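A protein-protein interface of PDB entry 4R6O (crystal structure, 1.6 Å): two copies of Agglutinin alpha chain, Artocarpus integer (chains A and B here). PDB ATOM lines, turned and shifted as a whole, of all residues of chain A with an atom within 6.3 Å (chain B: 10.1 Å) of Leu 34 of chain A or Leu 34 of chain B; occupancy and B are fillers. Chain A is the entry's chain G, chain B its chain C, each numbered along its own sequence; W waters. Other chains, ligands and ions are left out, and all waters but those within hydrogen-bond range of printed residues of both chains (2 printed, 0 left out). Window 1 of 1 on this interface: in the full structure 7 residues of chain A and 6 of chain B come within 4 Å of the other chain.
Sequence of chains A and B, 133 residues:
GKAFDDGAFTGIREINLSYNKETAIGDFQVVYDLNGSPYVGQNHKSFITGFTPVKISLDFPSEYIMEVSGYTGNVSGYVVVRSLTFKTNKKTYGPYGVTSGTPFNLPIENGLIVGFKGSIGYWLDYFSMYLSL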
ATOM      1  N   ALA A   8      10.533   3.856   8.102  1.00  0.00           N
ATOM      2  CA  ALA A   8      10.178   2.448   7.843  1.00  0.00           C
ATOM      3  C   ALA A   8      11.406   1.550   7.771  1.00  0.00           C
ATOM      4  O   ALA A   8      12.513   1.938   7.351  1.00  0.00           O
ATOM      5  CB  ALA A   8       9.463   2.350   6.498  1.00  0.00           C
ATOM      6  N   PHE A   9      11.181   0.331   8.244  1.00  0.00           N
ATOM      7  CA  PHE A   9      12.229  -0.710   8.396  1.00  0.00           C
ATOM      8  C   PHE A   9      11.789  -2.032   7.819  1.00  0.00           C
ATOM      9  O   PHE A   9      10.843  -2.083   7.032  1.00  0.00           O
ATOM     10  CB  PHE A   9      12.522  -0.791   9.906  1.00  0.00           C
ATOM     11  CG  PHE A   9      13.142   0.462  10.446  1.00  0.00           C
ATOM     12  CD1 PHE A   9      12.281   1.481  10.903  1.00  0.00           C
ATOM     13  CD2 PHE A   9      14.546   0.719  10.398  1.00  0.00           C
ATOM     14  CE1 PHE A   9      12.764   2.676  11.306  1.00  0.00           C
ATOM     15  CE2 PHE A   9      15.033   1.944  10.862  1.00  0.00           C
ATOM     16  CZ  PHE A   9      14.130   2.925  11.355  1.00  0.00           C
ATOM     17  N   THR A  10      12.477  -3.154   8.148  1.00  0.00           N
ATOM     18  CA  THR A  10      12.188  -4.431   7.573  1.00  0.00           C
ATOM     19  C   THR A  10      11.264  -5.248   8.474  1.00  0.00           C
ATOM     20  O   THR A  10      10.691  -6.186   8.024  1.00  0.00           O
ATOM     21  CB  THR A  10      13.511  -5.232   7.366  1.00  0.00           C
ATOM     22  OG1 THR A  10      14.481  -4.323   6.824  1.00  0.00           O
ATOM     23  CG2 THR A  10      13.332  -6.418   6.487  1.00  0.00           C
ATOM     24  N   GLY A  11      11.081  -4.784   9.710  1.00  0.00           N
ATOM     25  CA  GLY A  11      10.301  -5.599  10.662  1.00  0.00           C
ATOM     26  C   GLY A  11      10.508  -5.010  12.061  1.00  0.00           C
ATOM     27  O   GLY A  11      11.130  -3.966  12.272  1.00  0.00           O
ATOM     28  N   ARG A  13      11.574  -5.996  16.072  1.00  0.00           N
ATOM     29  CA  ARG A  13      12.179  -6.955  17.025  1.00  0.00           C
ATOM     30  C   ARG A  13      11.703  -6.745  18.472  1.00  0.00           C
ATOM     31  O   ARG A  13      11.453  -7.767  19.207  1.00  0.00           O
ATOM     32  CB  ARG A  13      13.682  -6.891  16.957  1.00  0.00           C
ATOM     33  CG  ARG A  13      14.215  -7.577  15.696  1.00  0.00           C
ATOM     34  CD  ARG A  13      15.615  -7.036  15.448  1.00  0.00           C
ATOM     35  NE  ARG A  13      16.259  -7.803  14.351  1.00  0.00           N
ATOM     36  CZ  ARG A  13      16.888  -8.965  14.471  1.00  0.00           C
ATOM     37  NH1 ARG A  13      16.956  -9.604  15.635  1.00  0.00           N
ATOM     38  NH2 ARG A  13      17.402  -9.518  13.369  1.00  0.00           N
ATOM     39  N   TYR A  32      13.882  -2.062  15.642  1.00  0.00           N
ATOM     40  CA  TYR A  32      13.399  -2.578  14.421  1.00  0.00           C
ATOM     41  C   TYR A  32      14.349  -3.672  13.888  1.00  0.00           C
ATOM     42  O   TYR A  32      15.468  -3.841  14.486  1.00  0.00           O
ATOM     43  CB  TYR A  32      13.332  -1.456  13.379  1.00  0.00           C
ATOM     44  CG  TYR A  32      12.343  -0.378  13.804  1.00  0.00           C
ATOM     45  CD1 TYR A  32      10.998  -0.536  13.471  1.00  0.00           C
ATOM     46  CD2 TYR A  32      12.817   0.792  14.395  1.00  0.00           C
ATOM     47  CE1 TYR A  32      10.068   0.463  13.821  1.00  0.00           C
ATOM     48  CE2 TYR A  32      11.898   1.799  14.764  1.00  0.00           C
ATOM     49  CZ  TYR A  32      10.530   1.600  14.426  1.00  0.00           C
ATOM     50  OH  TYR A  32       9.533   2.574  14.774  1.00  0.00           O
ATOM     51  N   ASP A  33      13.901  -4.364  12.873  1.00  0.00           N
ATOM     52  CA  ASP A  33      14.831  -5.152  12.056  1.00  0.00           C
ATOM     53  C   ASP A  33      15.211  -4.291  10.878  1.00  0.00           C
ATOM     54  O   ASP A  33      14.333  -3.666  10.245  1.00  0.00           O
ATOM     55  CB  ASP A  33      14.287  -6.462  11.583  1.00  0.00           C
ATOM     56  CG  ASP A  33      15.333  -7.206  10.788  1.00  0.00           C
ATOM     57  OD1 ASP A  33      16.228  -7.706  11.477  1.00  0.00           O
ATOM     58  OD2 ASP A  33      15.307  -7.238   9.519  1.00  0.00           O
ATOM     59  N   LEU A  34      16.502  -4.229  10.566  1.00  0.00           N
ATOM     60  CA  LEU A  34      16.934  -3.579   9.289  1.00  0.00           C
ATOM     61  C   LEU A  34      17.751  -4.627   8.520  1.00  0.00           C
ATOM     62  O   LEU A  34      18.930  -4.866   8.867  1.00  0.00           O
ATOM     63  CB  LEU A  34      17.724  -2.326   9.542  1.00  0.00           C
ATOM     64  CG  LEU A  34      18.214  -1.591   8.294  1.00  0.00           C
ATOM     65  CD1 LEU A  34      17.076  -1.075   7.405  1.00  0.00           C
ATOM     66  CD2 LEU A  34      19.173  -0.499   8.715  1.00  0.00           C
ATOM     67  N   ASN A  35      17.134  -5.204   7.495  1.00  0.00           N
ATOM     68  CA  ASN A  35      17.829  -6.168   6.597  1.00  0.00           C
ATOM     69  C   ASN A  35      18.583  -7.205   7.415  1.00  0.00           C
ATOM     70  O   ASN A  35      19.710  -7.588   7.102  1.00  0.00           O
ATOM     71  CB  ASN A  35      18.719  -5.363   5.661  1.00  0.00           C
ATOM     72  CG  ASN A  35      17.893  -4.425   4.841  1.00  0.00           C
ATOM     73  OD1 ASN A  35      16.846  -4.851   4.324  1.00  0.00           O
ATOM     74  ND2 ASN A  35      18.315  -3.173   4.707  1.00  0.00           N
ATOM     75  N   GLY A  36      17.940  -7.712   8.468  1.00  0.00           N
ATOM     76  CA  GLY A  36      18.533  -8.823   9.164  1.00  0.00           C
ATOM     77  C   GLY A  36      19.188  -8.461  10.466  1.00  0.00           C
ATOM     78  O   GLY A  36      19.389  -9.369  11.286  1.00  0.00           O
ATOM     79  N   SER A  37      19.554  -7.187  10.667  1.00  0.00           N
ATOM     80  CA  SER A  37      20.153  -6.749  11.916  1.00  0.00           C
ATOM     81  C   SER A  37      19.238  -5.914  12.813  1.00  0.00           C
ATOM     82  O   SER A  37      18.385  -5.225  12.298  1.00  0.00           O
ATOM     83  CB  SER A  37      21.370  -5.947  11.620  1.00  0.00           C
ATOM     84  OG  SER A  37      22.316  -6.889  11.071  1.00  0.00           O
ATOM     85  N   PRO A  38      19.447  -5.963  14.127  1.00  0.00           N
ATOM     86  CA  PRO A  38      18.670  -5.013  15.016  1.00  0.00           C
ATOM     87  C   PRO A  38      19.027  -3.585  14.705  1.00  0.00           C
ATOM     88  O   PRO A  38      20.205  -3.231  14.583  1.00  0.00           O
ATOM     89  CB  PRO A  38      19.105  -5.406  16.456  1.00  0.00           C
ATOM     90  CG  PRO A  38      19.735  -6.763  16.257  1.00  0.00           C
ATOM     91  CD  PRO A  38      20.450  -6.699  14.917  1.00  0.00           C
ATOM     92  N   TYR A  39      18.027  -2.699  14.621  1.00  0.00           N
ATOM     93  CA  TYR A  39      18.207  -1.300  14.530  1.00  0.00           C
ATOM     94  C   TYR A  39      17.569  -0.665  15.769  1.00  0.00           C
ATOM     95  O   TYR A  39      16.339  -0.801  16.004  1.00  0.00           O
ATOM     96  CB  TYR A  39      17.473  -0.802  13.282  1.00  0.00           C
ATOM     97  CG  TYR A  39      17.669   0.655  13.080  1.00  0.00           C
ATOM     98  CD1 TYR A  39      16.918   1.588  13.812  1.00  0.00           C
ATOM     99  CD2 TYR A  39      18.538   1.125  12.112  1.00  0.00           C
ATOM    100  CE1 TYR A  39      17.072   2.947  13.587  1.00  0.00           C
ATOM    101  CE2 TYR A  39      18.731   2.466  11.927  1.00  0.00           C
ATOM    102  CZ  TYR A  39      17.982   3.371  12.663  1.00  0.00           C
ATOM    103  OH  TYR A  39      18.087   4.728  12.493  1.00  0.00           O
ATOM    104  N   ASP B   5      24.689  -8.930   0.273  1.00  0.00           N
ATOM    105  CA  ASP B   5      23.293  -8.530   0.117  1.00  0.00           C
ATOM    106  C   ASP B   5      23.020  -7.397   1.077  1.00  0.00           C
ATOM    107  O   ASP B   5      22.903  -7.625   2.303  1.00  0.00           O
ATOM    108  CB  ASP B   5      22.389  -9.772   0.448  1.00  0.00           C
ATOM    109  CG  ASP B   5      20.930  -9.524   0.149  1.00  0.00           C
ATOM    110  OD1 ASP B   5      20.551  -8.341  -0.069  1.00  0.00           O
ATOM    111  OD2 ASP B   5      20.150 -10.498   0.189  1.00  0.00           O
ATOM    112  N   ASP B   6      22.980  -6.157   0.577  1.00  0.00           N
ATOM    113  CA  ASP B   6      22.735  -5.020   1.444  1.00  0.00           C
ATOM    114  C   ASP B   6      21.316  -4.960   1.997  1.00  0.00           C
ATOM    115  O   ASP B   6      21.063  -4.180   2.984  1.00  0.00           O
ATOM    116  CB  ASP B   6      22.977  -3.714   0.667  1.00  0.00           C
ATOM    117  CG  ASP B   6      24.494  -3.486   0.283  1.00  0.00           C
ATOM    118  OD1 ASP B   6      25.365  -4.154   0.914  1.00  0.00           O
ATOM    119  OD2 ASP B   6      24.784  -2.622  -0.568  1.00  0.00           O
ATOM    120  N   GLY B   7      20.382  -5.596   1.282  1.00  0.00           N
ATOM    121  CA  GLY B   7      18.932  -5.460   1.528  1.00  0.00           C
ATOM    122  C   GLY B   7      18.374  -4.144   1.002  1.00  0.00           C
ATOM    123  O   GLY B   7      18.982  -3.490   0.176  1.00  0.00           O
ATOM    124  N   ALA B   8      17.225  -3.714   1.515  1.00  0.00           N
ATOM    125  CA  ALA B   8      16.499  -2.568   0.901  1.00  0.00           C
ATOM    126  C   ALA B   8      16.523  -1.387   1.912  1.00  0.00           C
ATOM    127  O   ALA B   8      16.491  -1.574   3.153  1.00  0.00           O
ATOM    128  CB  ALA B   8      15.039  -3.007   0.682  1.00  0.00           C
ATOM    129  N   PHE B   9      16.573  -0.189   1.325  1.00  0.00           N
ATOM    130  CA  PHE B   9      16.641   1.065   2.044  1.00  0.00           C
ATOM    131  C   PHE B   9      15.615   2.016   1.468  1.00  0.00           C
ATOM    132  O   PHE B   9      14.695   1.579   0.783  1.00  0.00           O
ATOM    133  CB  PHE B   9      18.097   1.594   1.928  1.00  0.00           C
ATOM    134  CG  PHE B   9      19.067   0.744   2.664  1.00  0.00           C
ATOM    135  CD1 PHE B   9      19.679  -0.354   2.025  1.00  0.00           C
ATOM    136  CD2 PHE B   9      19.353   1.005   3.984  1.00  0.00           C
ATOM    137  CE1 PHE B   9      20.553  -1.214   2.719  1.00  0.00           C
ATOM    138  CE2 PHE B   9      20.224   0.163   4.661  1.00  0.00           C
ATOM    139  CZ  PHE B   9      20.864  -0.923   4.037  1.00  0.00           C
ATOM    140  N   THR B  10      15.755   3.334   1.772  1.00  0.00           N
ATOM    141  CA  THR B  10      14.825   4.352   1.302  1.00  0.00           C
ATOM    142  C   THR B  10      15.220   4.935  -0.041  1.00  0.00           C
ATOM    143  O   THR B  10      14.430   5.577  -0.734  1.00  0.00           O
ATOM    144  CB  THR B  10      14.730   5.525   2.361  1.00  0.00           C
ATOM    145  OG1 THR B  10      14.439   4.963   3.626  1.00  0.00           O
ATOM    146  CG2 THR B  10      13.665   6.540   1.958  1.00  0.00           C
ATOM    147  N   GLY B  11      16.458   4.724  -0.449  1.00  0.00           N
ATOM    148  CA  GLY B  11      16.906   5.419  -1.671  1.00  0.00           C
ATOM    149  C   GLY B  11      18.439   5.329  -1.727  1.00  0.00           C
ATOM    150  O   GLY B  11      19.058   4.660  -0.899  1.00  0.00           O
ATOM    151  N   ILE B  12      19.053   6.042  -2.693  1.00  0.00           N
ATOM    152  CA  ILE B  12      20.518   5.978  -2.853  1.00  0.00           C
ATOM    153  C   ILE B  12      21.131   7.391  -2.850  1.00  0.00           C
ATOM    154  O   ILE B  12      20.633   8.241  -3.566  1.00  0.00           O
ATOM    155  CB  ILE B  12      20.865   5.287  -4.182  1.00  0.00           C
ATOM    156  CG1 ILE B  12      20.424   3.799  -4.132  1.00  0.00           C
ATOM    157  CG2 ILE B  12      22.368   5.292  -4.462  1.00  0.00           C
ATOM    158  CD1 ILE B  12      20.600   3.070  -5.443  1.00  0.00           C
ATOM    159  N   ARG B  13      22.164   7.573  -2.056  1.00  0.00           N
ATOM    160  CA  ARG B  13      22.844   8.879  -1.979  1.00  0.00           C
ATOM    161  C   ARG B  13      24.154   8.888  -2.769  1.00  0.00           C
ATOM    162  O   ARG B  13      24.470   9.900  -3.438  1.00  0.00           O
ATOM    163  CB  ARG B  13      23.010   9.399  -0.542  1.00  0.00           C
ATOM    164  CG  ARG B  13      21.696   9.727   0.188  1.00  0.00           C
ATOM    165  CD  ARG B  13      21.940   9.762   1.671  1.00  0.00           C
ATOM    166  NE  ARG B  13      20.789  10.312   2.387  1.00  0.00           N
ATOM    167  CZ  ARG B  13      20.614  11.611   2.636  1.00  0.00           C
ATOM    168  NH1 ARG B  13      21.529  12.501   2.269  1.00  0.00           N
ATOM    169  NH2 ARG B  13      19.533  12.019   3.282  1.00  0.00           N
ATOM    170  N   GLU B  14      24.886   7.798  -2.738  1.00  0.00           N
ATOM    171  CA  GLU B  14      26.180   7.810  -3.413  1.00  0.00           C
ATOM    172  C   GLU B  14      26.538   6.396  -3.781  1.00  0.00           C
ATOM    173  O   GLU B  14      26.244   5.454  -3.062  1.00  0.00           O
ATOM    174  CB  GLU B  14      27.193   8.309  -2.412  1.00  0.00           C
ATOM    175  CG  GLU B  14      28.607   8.485  -2.905  1.00  0.00           C
ATOM    176  CD  GLU B  14      29.407   9.202  -1.823  1.00  0.00           C
ATOM    177  OE1 GLU B  14      29.329  10.464  -1.784  1.00  0.00           O
ATOM    178  OE2 GLU B  14      30.037   8.488  -0.995  1.00  0.00           O
ATOM    179  N   VAL B  30      27.710   1.268  -1.420  1.00  0.00           N
ATOM    180  CA  VAL B  30      26.663   2.252  -1.601  1.00  0.00           C
ATOM    181  C   VAL B  30      26.417   2.979  -0.292  1.00  0.00           C
ATOM    182  O   VAL B  30      26.369   2.371   0.787  1.00  0.00           O
ATOM    183  CB  VAL B  30      25.325   1.574  -2.063  1.00  0.00           C
ATOM    184  CG1 VAL B  30      24.260   2.652  -2.238  1.00  0.00           C
ATOM    185  CG2 VAL B  30      25.552   0.732  -3.327  1.00  0.00           C
ATOM    186  N   VAL B  31      26.259   4.301  -0.386  1.00  0.00           N
ATOM    187  CA  VAL B  31      25.712   5.125   0.711  1.00  0.00           C
ATOM    188  C   VAL B  31      24.228   5.263   0.375  1.00  0.00           C
ATOM    189  O   VAL B  31      23.816   5.908  -0.597  1.00  0.00           O
ATOM    190  CB  VAL B  31      26.323   6.544   0.800  1.00  0.00           C
ATOM    191  CG1 VAL B  31      25.691   7.299   1.938  1.00  0.00           C
ATOM    192  CG2 VAL B  31      27.817   6.478   1.043  1.00  0.00           C
ATOM    193  N   TYR B  32      23.395   4.606   1.181  1.00  0.00           N
ATOM    194  CA  TYR B  32      21.941   4.652   0.971  1.00  0.00           C
ATOM    195  C   TYR B  32      21.279   5.842   1.697  1.00  0.00           C
ATOM    196  O   TYR B  32      21.912   6.466   2.526  1.00  0.00           O
ATOM    197  CB  TYR B  32      21.343   3.343   1.549  1.00  0.00           C
ATOM    198  CG  TYR B  32      21.755   2.142   0.773  1.00  0.00           C
ATOM    199  CD1 TYR B  32      21.082   1.823  -0.397  1.00  0.00           C
ATOM    200  CD2 TYR B  32      22.740   1.268   1.257  1.00  0.00           C
ATOM    201  CE1 TYR B  32      21.458   0.729  -1.171  1.00  0.00           C
ATOM    202  CE2 TYR B  32      23.087   0.149   0.515  1.00  0.00           C
ATOM    203  CZ  TYR B  32      22.422  -0.113  -0.684  1.00  0.00           C
ATOM    204  OH  TYR B  32      22.735  -1.167  -1.498  1.00  0.00           O
ATOM    205  N   ASP B  33      20.060   6.144   1.330  1.00  0.00           N
ATOM    206  CA  ASP B  33      19.204   6.903   2.252  1.00  0.00           C
ATOM    207  C   ASP B  33      18.453   5.902   3.096  1.00  0.00           C
ATOM    208  O   ASP B  33      17.977   4.911   2.554  1.00  0.00           O
ATOM    209  CB  ASP B  33      18.267   7.818   1.522  1.00  0.00           C
ATOM    210  CG  ASP B  33      17.473   8.672   2.509  1.00  0.00           C
ATOM    211  OD1 ASP B  33      18.101   9.504   3.156  1.00  0.00           O
ATOM    212  OD2 ASP B  33      16.263   8.385   2.726  1.00  0.00           O
ATOM    213  N   LEU B  34      18.332   6.206   4.407  1.00  0.00           N
ATOM    214  CA  LEU B  34      17.431   5.476   5.266  1.00  0.00           C
ATOM    215  C   LEU B  34      16.606   6.499   6.027  1.00  0.00           C
ATOM    216  O   LEU B  34      17.099   7.149   6.968  1.00  0.00           O
ATOM    217  CB  LEU B  34      18.224   4.618   6.176  1.00  0.00           C
ATOM    218  CG  LEU B  34      17.382   3.756   7.178  1.00  0.00           C
ATOM    219  CD1 LEU B  34      16.522   2.750   6.425  1.00  0.00           C
ATOM    220  CD2 LEU B  34      18.363   3.074   8.149  1.00  0.00           C
ATOM    221  N   ASN B  35      15.348   6.558   5.635  1.00  0.00           N
ATOM    222  CA  ASN B  35      14.355   7.499   6.264  1.00  0.00           C
ATOM    223  C   ASN B  35      14.874   8.924   6.425  1.00  0.00           C
ATOM    224  O   ASN B  35      14.635   9.599   7.463  1.00  0.00           O
ATOM    225  CB  ASN B  35      13.903   6.882   7.593  1.00  0.00           C
ATOM    226  CG  ASN B  35      13.345   5.490   7.383  1.00  0.00           C
ATOM    227  OD1 ASN B  35      12.452   5.303   6.555  1.00  0.00           O
ATOM    228  ND2 ASN B  35      13.801   4.539   8.210  1.00  0.00           N
ATOM    229  N   GLY B  36      15.557   9.396   5.378  1.00  0.00           N
ATOM    230  CA  GLY B  36      16.049  10.784   5.364  1.00  0.00           C
ATOM    231  C   GLY B  36      17.444  11.048   5.880  1.00  0.00           C
ATOM    232  O   GLY B  36      17.877  12.207   5.838  1.00  0.00           O
ATOM    233  N   SER B  37      18.137  10.021   6.389  1.00  0.00           N
ATOM    234  CA  SER B  37      19.490  10.133   6.888  1.00  0.00           C
ATOM    235  C   SER B  37      20.374   9.191   6.066  1.00  0.00           C
ATOM    236  O   SER B  37      19.918   8.131   5.627  1.00  0.00           O
ATOM    237  CB  SER B  37      19.626   9.732   8.367  1.00  0.00           C
ATOM    238  OG  SER B  37      18.765  10.499   9.198  1.00  0.00           O
ATOM    239  N   PRO B  38      21.635   9.558   5.857  1.00  0.00           N
ATOM    240  CA  PRO B  38      22.510   8.656   5.140  1.00  0.00           C
ATOM    241  C   PRO B  38      22.820   7.385   5.940  1.00  0.00           C
ATOM    242  O   PRO B  38      22.815   7.396   7.170  1.00  0.00           O
ATOM    243  CB  PRO B  38      23.761   9.533   4.822  1.00  0.00           C
ATOM    244  CG  PRO B  38      23.712  10.629   5.845  1.00  0.00           C
ATOM    245  CD  PRO B  38      22.244  10.890   6.096  1.00  0.00           C
ATOM    246  N   TYR B  39      22.980   6.270   5.230  1.00  0.00           N
ATOM    247  CA  TYR B  39      23.346   4.987   5.829  1.00  0.00           C
ATOM    248  C   TYR B  39      24.476   4.433   5.000  1.00  0.00           C
ATOM    249  O   TYR B  39      24.304   4.185   3.789  1.00  0.00           O
ATOM    250  CB  TYR B  39      22.147   4.066   5.829  1.00  0.00           C
ATOM    251  CG  TYR B  39      22.487   2.756   6.435  1.00  0.00           C
ATOM    252  CD1 TYR B  39      23.051   1.769   5.672  1.00  0.00           C
ATOM    253  CD2 TYR B  39      22.337   2.559   7.836  1.00  0.00           C
ATOM    254  CE1 TYR B  39      23.390   0.536   6.231  1.00  0.00           C
ATOM    255  CE2 TYR B  39      22.701   1.365   8.394  1.00  0.00           C
ATOM    256  CZ  TYR B  39      23.222   0.375   7.606  1.00  0.00           C
ATOM    257  OH  TYR B  39      23.578  -0.829   8.211  1.00  0.00           O
ATOM    258  N   VAL B  40      25.655   4.279   5.619  1.00  0.00           N
ATOM    259  CA  VAL B  40      26.861   3.887   4.850  1.00  0.00           C
ATOM    260  C   VAL B  40      26.832   2.339   4.741  1.00  0.00           C
ATOM    261  O   VAL B  40      26.956   1.572   5.754  1.00  0.00           O
ATOM    262  CB  VAL B  40      28.177   4.427   5.492  1.00  0.00           C
ATOM    263  CG1 VAL B  40      29.392   3.930   4.720  1.00  0.00           C
ATOM    264  CG2 VAL B  40      28.154   5.989   5.580  1.00  0.00           C
ATOM    265  N   GLY B  41      26.611   1.845   3.521  1.00  0.00           N
ATOM    266  CA  GLY B  41      26.602   0.401   3.244  1.00  0.00           C
ATOM    267  C   GLY B  41      27.955  -0.271   3.459  1.00  0.00           C
ATOM    268  O   GLY B  41      28.983   0.422   3.506  1.00  0.00           O
ATOM    269  N   PHE B  60      20.746  13.671  -3.940  1.00  0.00           N
ATOM    270  CA  PHE B  60      19.560  13.120  -3.308  1.00  0.00           C
ATOM    271  C   PHE B  60      18.792  14.196  -2.531  1.00  0.00           C
ATOM    272  O   PHE B  60      19.399  15.024  -1.887  1.00  0.00           O
ATOM    273  CB  PHE B  60      20.005  12.010  -2.364  1.00  0.00           C
ATOM    274  CG  PHE B  60      18.865  11.338  -1.628  1.00  0.00           C
ATOM    275  CD1 PHE B  60      18.398  11.873  -0.421  1.00  0.00           C
ATOM    276  CD2 PHE B  60      18.206  10.224  -2.189  1.00  0.00           C
ATOM    277  CE1 PHE B  60      17.340  11.253   0.258  1.00  0.00           C
ATOM    278  CE2 PHE B  60      17.143   9.621  -1.533  1.00  0.00           C
ATOM    279  CZ  PHE B  60      16.711  10.152  -0.311  1.00  0.00           C
ATOM    280  N   VAL B 114      16.513   0.498  -4.562  1.00  0.00           N
ATOM    281  CA  VAL B 114      16.708   0.775  -3.142  1.00  0.00           C
ATOM    282  C   VAL B 114      17.663  -0.200  -2.479  1.00  0.00           C
ATOM    283  O   VAL B 114      17.732  -0.246  -1.243  1.00  0.00           O
ATOM    284  CB  VAL B 114      15.313   0.798  -2.419  1.00  0.00           C
ATOM    285  CG1 VAL B 114      14.412   1.872  -3.029  1.00  0.00           C
ATOM    286  CG2 VAL B 114      14.647  -0.563  -2.545  1.00  0.00           C
ATOM    287  N   TYR B 130      17.263  -4.422  -5.652  1.00  0.00           N
ATOM    288  CA  TYR B 130      15.904  -4.297  -5.039  1.00  0.00           C
ATOM    289  C   TYR B 130      15.212  -3.059  -5.650  1.00  0.00           C
ATOM    290  O   TYR B 130      15.844  -2.003  -5.744  1.00  0.00           O
ATOM    291  CB  TYR B 130      16.076  -3.975  -3.612  1.00  0.00           C
ATOM    292  CG  TYR B 130      16.605  -5.134  -2.800  1.00  0.00           C
ATOM    293  CD1 TYR B 130      17.968  -5.507  -2.847  1.00  0.00           C
ATOM    294  CD2 TYR B 130      15.761  -5.819  -1.897  1.00  0.00           C
ATOM    295  CE1 TYR B 130      18.468  -6.586  -2.083  1.00  0.00           C
ATOM    296  CE2 TYR B 130      16.236  -6.919  -1.132  1.00  0.00           C
ATOM    297  CZ  TYR B 130      17.588  -7.260  -1.196  1.00  0.00           C
ATOM    298  OH  TYR B 130      18.039  -8.276  -0.409  1.00  0.00           O
HETATM  299  O   HOH W   1      14.484  -2.798   4.645  1.00  0.00           O
HETATM  300  O   HOH W   2      16.180   5.635  10.070  1.00  0.00           O
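Water W1 lies within hydrogen-bond range of the side-chain hydroxyl of Thr 10 of chain A, the backbone carbonyl oxygen of Ala 8 of chain B and the side-chain amide oxygen of Asn 35 of chain A. Water W2 lies within hydrogen-bond range of ND2 of Asn 35 of chain B (3.2 Å) and OH of Tyr 39 of chain A (3.2 Å).
Ala 8 of chain A touches Asn 35 of chain B, and with the chains exchanged Asn 35 of chain A touches Ala 8 of chain B. Phe 9 of chain A touches Asn 35 of chain B, and with the chains exchanged Asn 35 of chain A touches Phe 9 of chain B. Leu 34 of chain A touches its own counterpart, Leu 34 of chain B. Tyr 39 of chain A touches Leu 34 of chain B, but with the chains exchanged Leu 34 of chain A does not touch Tyr 39 of chain B (4.003 Å). 13 positions are printed for both chains.
Printed residues of chain B within 4 Å of Leu 34 of chain A: Leu 34. Printed residues of chain A within 4 Å of Leu 34 of chain B: Leu 34 and Tyr 39. No residue of chain B comes within 4 Å of Asp 33 of chain A. No residue of chain B comes within 4 Å of Gly 36 of chain A. No residue of chain B comes within 4 Å of Ser 37 of chain A. Of the printed residues of chain A, Asp 6 of chain B touches Asn 35. Of the printed residues of chain A, Asn 35 of chain B touches Ala 8 and Phe 9. Of the printed residues of chain B, Ala 8 of chain A touches Asn 35. Thr 10 of chain B touches none of the printed residues of chain A. Tyr 39 of chain B touches none of the printed residues of chain A. The nearest residue of chain A that does not touch Leu 34 of chain B is Ala 8 of chain A (4.2 Å).
Printed residues of chain B that touch a printed residue of chain A: Asp 6, Gly 7, Ala 8, Phe 9, Leu 34 and Asn 35. Hydrophobic or aromatic side chains of chain A that line the printed part of chain B: Phe 9, Leu 34 and Tyr 39. Among the printed residues, 8 pairs touch across the chains. Among the printed residues, no Asp or Glu carboxylate lies within 4 Å of a Lys or Arg side-chain nitrogen of the other chain.
Asn 35 of chain B touches Phe 9 of chain A. CD2 of Leu 34 of chain B touches CD2 of Leu 34 of chain A, 3.7 Å away. OD1 of Asn 35 of chain A touches CA of Gly 7 of chain B (3.5 Å). Asn 35 of chain A touches Phe 9 of chain B. Tyr 39 of chain A touches Leu 34 of chain B.
O of Asp 6 of chain B is in hydrogen-bond range of ND2 of Asn 35 of chain A, at 3.4 Å. The side-chain amide oxygen (OD1) of Asn 35 of chain B is in hydrogen-bond range of the backbone NH (N) of Ala 8 of chain A (2.9 Å). O of Ala 8 of chain B is in hydrogen-bond range of ND2 of Asn 35 of chain A (2.9 Å).
N of Asn 35 of chain B sits at hydrogen-bond distance from OG1 of Thr 10 of chain B. The backbone NH (N) of Asn 35 of chain A is in hydrogen-bond range of the side-chain hydroxyl (OG1) of Thr 10 of chain A (2.9 Å). The side-chain hydroxyl (OH) of Tyr 32 of chain B sits at hydrogen-bond distance from the side-chain carboxylate (OD2) of Asp 6 of chain B (2.7 Å). The side-chain carboxylate (OD2) of Asp 33 of chain A lies within hydrogen-bond range of the backbone NH (N) of Asn 35 of chain A (3.4 Å). N of Tyr 32 of chain A lies within hydrogen-bond range of O of Tyr 39 of chain A. OD1 of Asp 5 of chain B lies within hydrogen-bond range of N of Gly 7 of chain B (3.1 Å).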
